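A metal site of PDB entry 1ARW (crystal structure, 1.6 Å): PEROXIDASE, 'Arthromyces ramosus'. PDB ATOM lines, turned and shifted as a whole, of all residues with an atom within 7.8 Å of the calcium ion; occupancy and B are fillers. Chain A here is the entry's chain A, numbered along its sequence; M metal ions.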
ATOM      1  N   PRO A 130     -25.950 -23.542 -18.629  1.00  0.00           N
ATOM      2  CA  PRO A 130     -24.862 -23.134 -17.747  1.00  0.00           C
ATOM      3  C   PRO A 130     -25.142 -21.843 -16.988  1.00  0.00           C
ATOM      4  O   PRO A 130     -25.656 -20.877 -17.563  1.00  0.00           O
ATOM      5  CB  PRO A 130     -23.683 -23.006 -18.660  1.00  0.00           C
ATOM      6  CG  PRO A 130     -23.990 -24.022 -19.747  1.00  0.00           C
ATOM      7  CD  PRO A 130     -25.468 -23.797 -19.975  1.00  0.00           C
ATOM      8  N   ALA A 182     -34.654 -11.701 -16.042  1.00  0.00           N
ATOM      9  CA  ALA A 182     -33.379 -12.364 -16.232  1.00  0.00           C
ATOM     10  C   ALA A 182     -33.590 -13.515 -17.227  1.00  0.00           C
ATOM     11  O   ALA A 182     -32.655 -13.914 -17.921  1.00  0.00           O
ATOM     12  CB  ALA A 182     -32.834 -12.951 -14.934  1.00  0.00           C
ATOM     13  N   ALA A 183     -34.801 -14.050 -17.380  1.00  0.00           N
ATOM     14  CA  ALA A 183     -35.051 -15.091 -18.344  1.00  0.00           C
ATOM     15  C   ALA A 183     -34.760 -14.652 -19.782  1.00  0.00           C
ATOM     16  O   ALA A 183     -34.480 -15.514 -20.622  1.00  0.00           O
ATOM     17  CB  ALA A 183     -36.487 -15.521 -18.232  1.00  0.00           C
ATOM     18  N   HIS A 184     -34.708 -13.360 -20.127  1.00  0.00           N
ATOM     19  CA  HIS A 184     -34.342 -12.907 -21.476  1.00  0.00           C
ATOM     20  C   HIS A 184     -32.817 -13.031 -21.748  1.00  0.00           C
ATOM     21  O   HIS A 184     -32.300 -12.667 -22.821  1.00  0.00           O
ATOM     22  CB  HIS A 184     -34.834 -11.451 -21.675  1.00  0.00           C
ATOM     23  CG  HIS A 184     -36.320 -11.321 -22.060  1.00  0.00           C
ATOM     24  ND1 HIS A 184     -36.911 -10.143 -22.495  1.00  0.00           N
ATOM     25  CD2 HIS A 184     -37.282 -12.328 -22.059  1.00  0.00           C
ATOM     26  CE1 HIS A 184     -38.184 -10.417 -22.812  1.00  0.00           C
ATOM     27  NE2 HIS A 184     -38.427 -11.668 -22.551  1.00  0.00           N
ATOM     28  N   SER A 185     -32.061 -13.536 -20.752  1.00  0.00           N
ATOM     29  CA  SER A 185     -30.654 -13.855 -20.933  1.00  0.00           C
ATOM     30  C   SER A 185     -30.620 -15.211 -21.647  1.00  0.00           C
ATOM     31  O   SER A 185     -29.530 -15.609 -22.085  1.00  0.00           O
ATOM     32  CB  SER A 185     -29.967 -13.947 -19.565  1.00  0.00           C
ATOM     33  OG  SER A 185     -28.555 -14.203 -19.665  1.00  0.00           O
ATOM     34  N   LEU A 186     -31.705 -15.959 -21.844  1.00  0.00           N
ATOM     35  CA  LEU A 186     -31.740 -17.268 -22.504  1.00  0.00           C
ATOM     36  C   LEU A 186     -32.848 -17.101 -23.539  1.00  0.00           C
ATOM     37  O   LEU A 186     -33.863 -17.801 -23.552  1.00  0.00           O
ATOM     38  CB  LEU A 186     -32.092 -18.280 -21.420  1.00  0.00           C
ATOM     39  CG  LEU A 186     -31.180 -19.334 -20.779  1.00  0.00           C
ATOM     40  CD1 LEU A 186     -29.739 -18.942 -20.806  1.00  0.00           C
ATOM     41  CD2 LEU A 186     -31.788 -19.639 -19.423  1.00  0.00           C
ATOM     42  N   ALA A 187     -32.683 -16.179 -24.480  1.00  0.00           N
ATOM     43  CA  ALA A 187     -33.787 -15.819 -25.374  1.00  0.00           C
ATOM     44  C   ALA A 187     -33.450 -15.340 -26.756  1.00  0.00           C
ATOM     45  O   ALA A 187     -32.371 -14.795 -27.042  1.00  0.00           O
ATOM     46  CB  ALA A 187     -34.598 -14.685 -24.694  1.00  0.00           C
ATOM     47  N   LEU A 201     -31.455 -12.185 -27.795  1.00  0.00           N
ATOM     48  CA  LEU A 201     -31.688 -10.956 -27.072  1.00  0.00           C
ATOM     49  C   LEU A 201     -30.401 -10.597 -26.327  1.00  0.00           C
ATOM     50  O   LEU A 201     -30.268  -9.484 -25.824  1.00  0.00           O
ATOM     51  CB  LEU A 201     -32.913 -11.166 -26.151  1.00  0.00           C
ATOM     52  CG  LEU A 201     -34.320 -10.687 -26.659  1.00  0.00           C
ATOM     53  CD1 LEU A 201     -34.580 -11.052 -28.103  1.00  0.00           C
ATOM     54  CD2 LEU A 201     -35.347 -11.239 -25.689  1.00  0.00           C
ATOM     55  N   ASP A 202     -29.419 -11.484 -26.126  1.00  0.00           N
ATOM     56  CA  ASP A 202     -28.147 -11.050 -25.563  1.00  0.00           C
ATOM     57  C   ASP A 202     -27.106 -11.900 -26.287  1.00  0.00           C
ATOM     58  O   ASP A 202     -27.517 -12.809 -27.017  1.00  0.00           O
ATOM     59  CB  ASP A 202     -28.030 -11.233 -24.024  1.00  0.00           C
ATOM     60  CG  ASP A 202     -27.827 -12.584 -23.344  1.00  0.00           C
ATOM     61  OD1 ASP A 202     -27.740 -13.626 -23.996  1.00  0.00           O
ATOM     62  OD2 ASP A 202     -27.773 -12.560 -22.115  1.00  0.00           O
ATOM     63  N   SER A 203     -25.815 -11.677 -26.078  1.00  0.00           N
ATOM     64  CA  SER A 203     -24.839 -12.459 -26.820  1.00  0.00           C
ATOM     65  C   SER A 203     -24.566 -13.875 -26.326  1.00  0.00           C
ATOM     66  O   SER A 203     -23.723 -14.577 -26.892  1.00  0.00           O
ATOM     67  CB  SER A 203     -23.553 -11.650 -26.865  1.00  0.00           C
ATOM     68  OG  SER A 203     -23.091 -11.363 -25.551  1.00  0.00           O
ATOM     69  N   THR A 204     -25.191 -14.347 -25.239  1.00  0.00           N
ATOM     70  CA  THR A 204     -24.983 -15.695 -24.764  1.00  0.00           C
ATOM     71  C   THR A 204     -26.352 -16.318 -24.553  1.00  0.00           C
ATOM     72  O   THR A 204     -26.738 -16.538 -23.404  1.00  0.00           O
ATOM     73  CB  THR A 204     -24.174 -15.640 -23.456  1.00  0.00           C
ATOM     74  OG1 THR A 204     -24.845 -14.716 -22.594  1.00  0.00           O
ATOM     75  CG2 THR A 204     -22.762 -15.187 -23.659  1.00  0.00           C
ATOM     76  N   PRO A 205     -27.152 -16.634 -25.586  1.00  0.00           N
ATOM     77  CA  PRO A 205     -28.488 -17.204 -25.415  1.00  0.00           C
ATOM     78  C   PRO A 205     -28.506 -18.584 -24.780  1.00  0.00           C
ATOM     79  O   PRO A 205     -29.593 -19.118 -24.491  1.00  0.00           O
ATOM     80  CB  PRO A 205     -29.066 -17.166 -26.801  1.00  0.00           C
ATOM     81  CG  PRO A 205     -27.834 -17.359 -27.668  1.00  0.00           C
ATOM     82  CD  PRO A 205     -26.882 -16.379 -26.994  1.00  0.00           C
ATOM     83  N   GLN A 206     -27.318 -19.201 -24.643  1.00  0.00           N
ATOM     84  CA  GLN A 206     -27.222 -20.485 -23.977  1.00  0.00           C
ATOM     85  C   GLN A 206     -26.563 -20.364 -22.617  1.00  0.00           C
ATOM     86  O   GLN A 206     -26.265 -21.396 -22.028  1.00  0.00           O
ATOM     87  CB  GLN A 206     -26.448 -21.482 -24.846  1.00  0.00           C
ATOM     88  CG  GLN A 206     -27.233 -21.922 -26.085  1.00  0.00           C
ATOM     89  CD  GLN A 206     -26.530 -23.043 -26.864  1.00  0.00           C
ATOM     90  OE1 GLN A 206     -25.470 -22.851 -27.444  1.00  0.00           O
ATOM     91  NE2 GLN A 206     -27.094 -24.250 -26.917  1.00  0.00           N
ATOM     92  N   VAL A 207     -26.271 -19.197 -22.049  1.00  0.00           N
ATOM     93  CA  VAL A 207     -25.687 -19.138 -20.723  1.00  0.00           C
ATOM     94  C   VAL A 207     -26.592 -18.235 -19.853  1.00  0.00           C
ATOM     95  O   VAL A 207     -26.959 -17.142 -20.327  1.00  0.00           O
ATOM     96  CB  VAL A 207     -24.234 -18.551 -20.777  1.00  0.00           C
ATOM     97  CG1 VAL A 207     -23.641 -18.441 -19.386  1.00  0.00           C
ATOM     98  CG2 VAL A 207     -23.363 -19.449 -21.608  1.00  0.00           C
ATOM     99  N   PHE A 208     -26.991 -18.577 -18.617  1.00  0.00           N
ATOM    100  CA  PHE A 208     -27.822 -17.708 -17.796  1.00  0.00           C
ATOM    101  C   PHE A 208     -26.827 -16.817 -17.070  1.00  0.00           C
ATOM    102  O   PHE A 208     -26.147 -17.221 -16.104  1.00  0.00           O
ATOM    103  CB  PHE A 208     -28.635 -18.529 -16.808  1.00  0.00           C
ATOM    104  CG  PHE A 208     -29.630 -17.748 -15.948  1.00  0.00           C
ATOM    105  CD1 PHE A 208     -30.770 -17.196 -16.504  1.00  0.00           C
ATOM    106  CD2 PHE A 208     -29.386 -17.627 -14.592  1.00  0.00           C
ATOM    107  CE1 PHE A 208     -31.653 -16.520 -15.701  1.00  0.00           C
ATOM    108  CE2 PHE A 208     -30.275 -16.952 -13.802  1.00  0.00           C
ATOM    109  CZ  PHE A 208     -31.406 -16.410 -14.361  1.00  0.00           C
ATOM    110  N   ASP A 209     -26.762 -15.595 -17.536  1.00  0.00           N
ATOM    111  CA  ASP A 209     -25.821 -14.608 -17.060  1.00  0.00           C
ATOM    112  C   ASP A 209     -26.402 -13.197 -17.162  1.00  0.00           C
ATOM    113  O   ASP A 209     -27.464 -12.887 -17.670  1.00  0.00           O
ATOM    114  CB  ASP A 209     -24.520 -14.694 -17.899  1.00  0.00           C
ATOM    115  CG  ASP A 209     -24.671 -14.494 -19.408  1.00  0.00           C
ATOM    116  OD1 ASP A 209     -25.750 -14.116 -19.901  1.00  0.00           O
ATOM    117  OD2 ASP A 209     -23.704 -14.788 -20.127  1.00  0.00           O
ATOM    118  N   THR A 210     -25.572 -12.306 -16.742  1.00  0.00           N
ATOM    119  CA  THR A 210     -25.845 -10.899 -16.690  1.00  0.00           C
ATOM    120  C   THR A 210     -25.783 -10.156 -18.038  1.00  0.00           C
ATOM    121  O   THR A 210     -26.184  -8.978 -18.116  1.00  0.00           O
ATOM    122  CB  THR A 210     -24.817 -10.624 -15.590  1.00  0.00           C
ATOM    123  OG1 THR A 210     -25.537 -10.368 -14.384  1.00  0.00           O
ATOM    124  CG2 THR A 210     -23.775  -9.749 -16.116  1.00  0.00           C
ATOM    125  N   GLN A 211     -25.352 -10.777 -19.148  1.00  0.00           N
ATOM    126  CA  GLN A 211     -25.181 -10.052 -20.406  1.00  0.00           C
ATOM    127  C   GLN A 211     -26.419  -9.340 -20.912  1.00  0.00           C
ATOM    128  O   GLN A 211     -26.264  -8.242 -21.463  1.00  0.00           O
ATOM    129  CB  GLN A 211     -24.667 -10.983 -21.508  1.00  0.00           C
ATOM    130  CG  GLN A 211     -23.225 -11.451 -21.312  1.00  0.00           C
ATOM    131  CD  GLN A 211     -22.193 -10.356 -21.044  1.00  0.00           C
ATOM    132  OE1 GLN A 211     -21.428 -10.434 -20.079  1.00  0.00           O
ATOM    133  NE2 GLN A 211     -22.094  -9.315 -21.832  1.00  0.00           N
ATOM    134  N   PHE A 212     -27.612  -9.867 -20.730  1.00  0.00           N
ATOM    135  CA  PHE A 212     -28.856  -9.224 -21.147  1.00  0.00           C
ATOM    136  C   PHE A 212     -29.008  -7.847 -20.504  1.00  0.00           C
ATOM    137  O   PHE A 212     -29.363  -6.900 -21.205  1.00  0.00           O
ATOM    138  CB  PHE A 212     -30.055 -10.097 -20.782  1.00  0.00           C
ATOM    139  CG  PHE A 212     -31.403  -9.403 -20.925  1.00  0.00           C
ATOM    140  CD1 PHE A 212     -31.895  -9.032 -22.172  1.00  0.00           C
ATOM    141  CD2 PHE A 212     -32.104  -9.101 -19.769  1.00  0.00           C
ATOM    142  CE1 PHE A 212     -33.106  -8.357 -22.231  1.00  0.00           C
ATOM    143  CE2 PHE A 212     -33.304  -8.429 -19.847  1.00  0.00           C
ATOM    144  CZ  PHE A 212     -33.806  -8.055 -21.074  1.00  0.00           C
ATOM    145  N   TYR A 213     -28.690  -7.688 -19.229  1.00  0.00           N
ATOM    146  CA  TYR A 213     -28.831  -6.391 -18.581  1.00  0.00           C
ATOM    147  C   TYR A 213     -27.813  -5.391 -19.107  1.00  0.00           C
ATOM    148  O   TYR A 213     -28.142  -4.235 -19.397  1.00  0.00           O
ATOM    149  CB  TYR A 213     -28.700  -6.606 -17.079  1.00  0.00           C
ATOM    150  CG  TYR A 213     -29.895  -7.394 -16.492  1.00  0.00           C
ATOM    151  CD1 TYR A 213     -31.130  -6.795 -16.327  1.00  0.00           C
ATOM    152  CD2 TYR A 213     -29.719  -8.709 -16.104  1.00  0.00           C
ATOM    153  CE1 TYR A 213     -32.199  -7.489 -15.777  1.00  0.00           C
ATOM    154  CE2 TYR A 213     -30.787  -9.414 -15.547  1.00  0.00           C
ATOM    155  CZ  TYR A 213     -32.025  -8.798 -15.381  1.00  0.00           C
ATOM    156  OH  TYR A 213     -33.056  -9.516 -14.809  1.00  0.00           O
ATOM    157  N   GLU A 215     -26.127  -5.451 -22.111  1.00  0.00           N
ATOM    158  CA  GLU A 215     -26.318  -5.132 -23.510  1.00  0.00           C
ATOM    159  C   GLU A 215     -27.585  -4.366 -23.864  1.00  0.00           C
ATOM    160  O   GLU A 215     -27.520  -3.659 -24.878  1.00  0.00           O
ATOM    161  CB  GLU A 215     -26.200  -6.427 -24.295  1.00  0.00           C
ATOM    162  CG  GLU A 215     -24.825  -7.066 -24.135  1.00  0.00           C
ATOM    163  CD  GLU A 215     -24.698  -8.480 -24.687  1.00  0.00           C
ATOM    164  OE1 GLU A 215     -25.538  -8.944 -25.465  1.00  0.00           O
ATOM    165  OE2 GLU A 215     -23.756  -9.146 -24.311  1.00  0.00           O
ATOM    166  N   ASN A 266     -23.505 -12.347 -11.432  1.00  0.00           N
ATOM    167  CA  ASN A 266     -24.329 -13.455 -11.834  1.00  0.00           C
ATOM    168  C   ASN A 266     -24.934 -14.081 -10.597  1.00  0.00           C
ATOM    169  O   ASN A 266     -26.038 -14.653 -10.611  1.00  0.00           O
ATOM    170  CB  ASN A 266     -23.519 -14.523 -12.531  1.00  0.00           C
ATOM    171  CG  ASN A 266     -23.152 -14.132 -13.949  1.00  0.00           C
ATOM    172  OD1 ASN A 266     -23.985 -13.647 -14.706  1.00  0.00           O
ATOM    173  ND2 ASN A 266     -21.925 -14.372 -14.392  1.00  0.00           N
ATOM    174  N   MET A 269     -27.950 -11.905  -9.440  1.00  0.00           N
ATOM    175  CA  MET A 269     -29.007 -12.107 -10.412  1.00  0.00           C
ATOM    176  C   MET A 269     -29.703 -13.465 -10.212  1.00  0.00           C
ATOM    177  O   MET A 269     -30.923 -13.532 -10.100  1.00  0.00           O
ATOM    178  CB  MET A 269     -28.401 -12.004 -11.831  1.00  0.00           C
ATOM    179  CG  MET A 269     -29.453 -12.237 -12.890  1.00  0.00           C
ATOM    180  SD  MET A 269     -28.765 -12.411 -14.550  1.00  0.00           S
ATOM    181  CE  MET A 269     -28.259 -14.096 -14.406  1.00  0.00           C
HETATM  182 CA    CA M   1     -27.211 -14.886 -21.638  1.00  0.00          CA
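The side-chain carboxylate (OD1) of Asp 209 sits close to the backbone NH (N) of Gln 211 (3.4 Å).
The side-chain carboxylate (OD2) of Asp 202 lies close to the backbone NH (N) of Phe 212 (3.0 Å).
Within 4 Å of the calcium ion: Ser 185, Asp 202, Thr 204, Val 207 and Asp 209.
The nearest printed residue that does not touch the calcium ion is Pro 205 (4.3 Å).
The calcium ion is bound by OD1 of Asp 209 (2.4 Å), OD2 of Asp 202 (2.4 Å), O of Thr 204 (2.5 Å), O of Ser 185 (2.5 Å), OG of Ser 185 (2.5 Å), OG1 of Thr 204 (2.6 Å), O of Val 207 (2.6 Å) and OD1 of Asp 202 (2.7 Å).
The calcium ion has eight donor atoms within binding distance.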
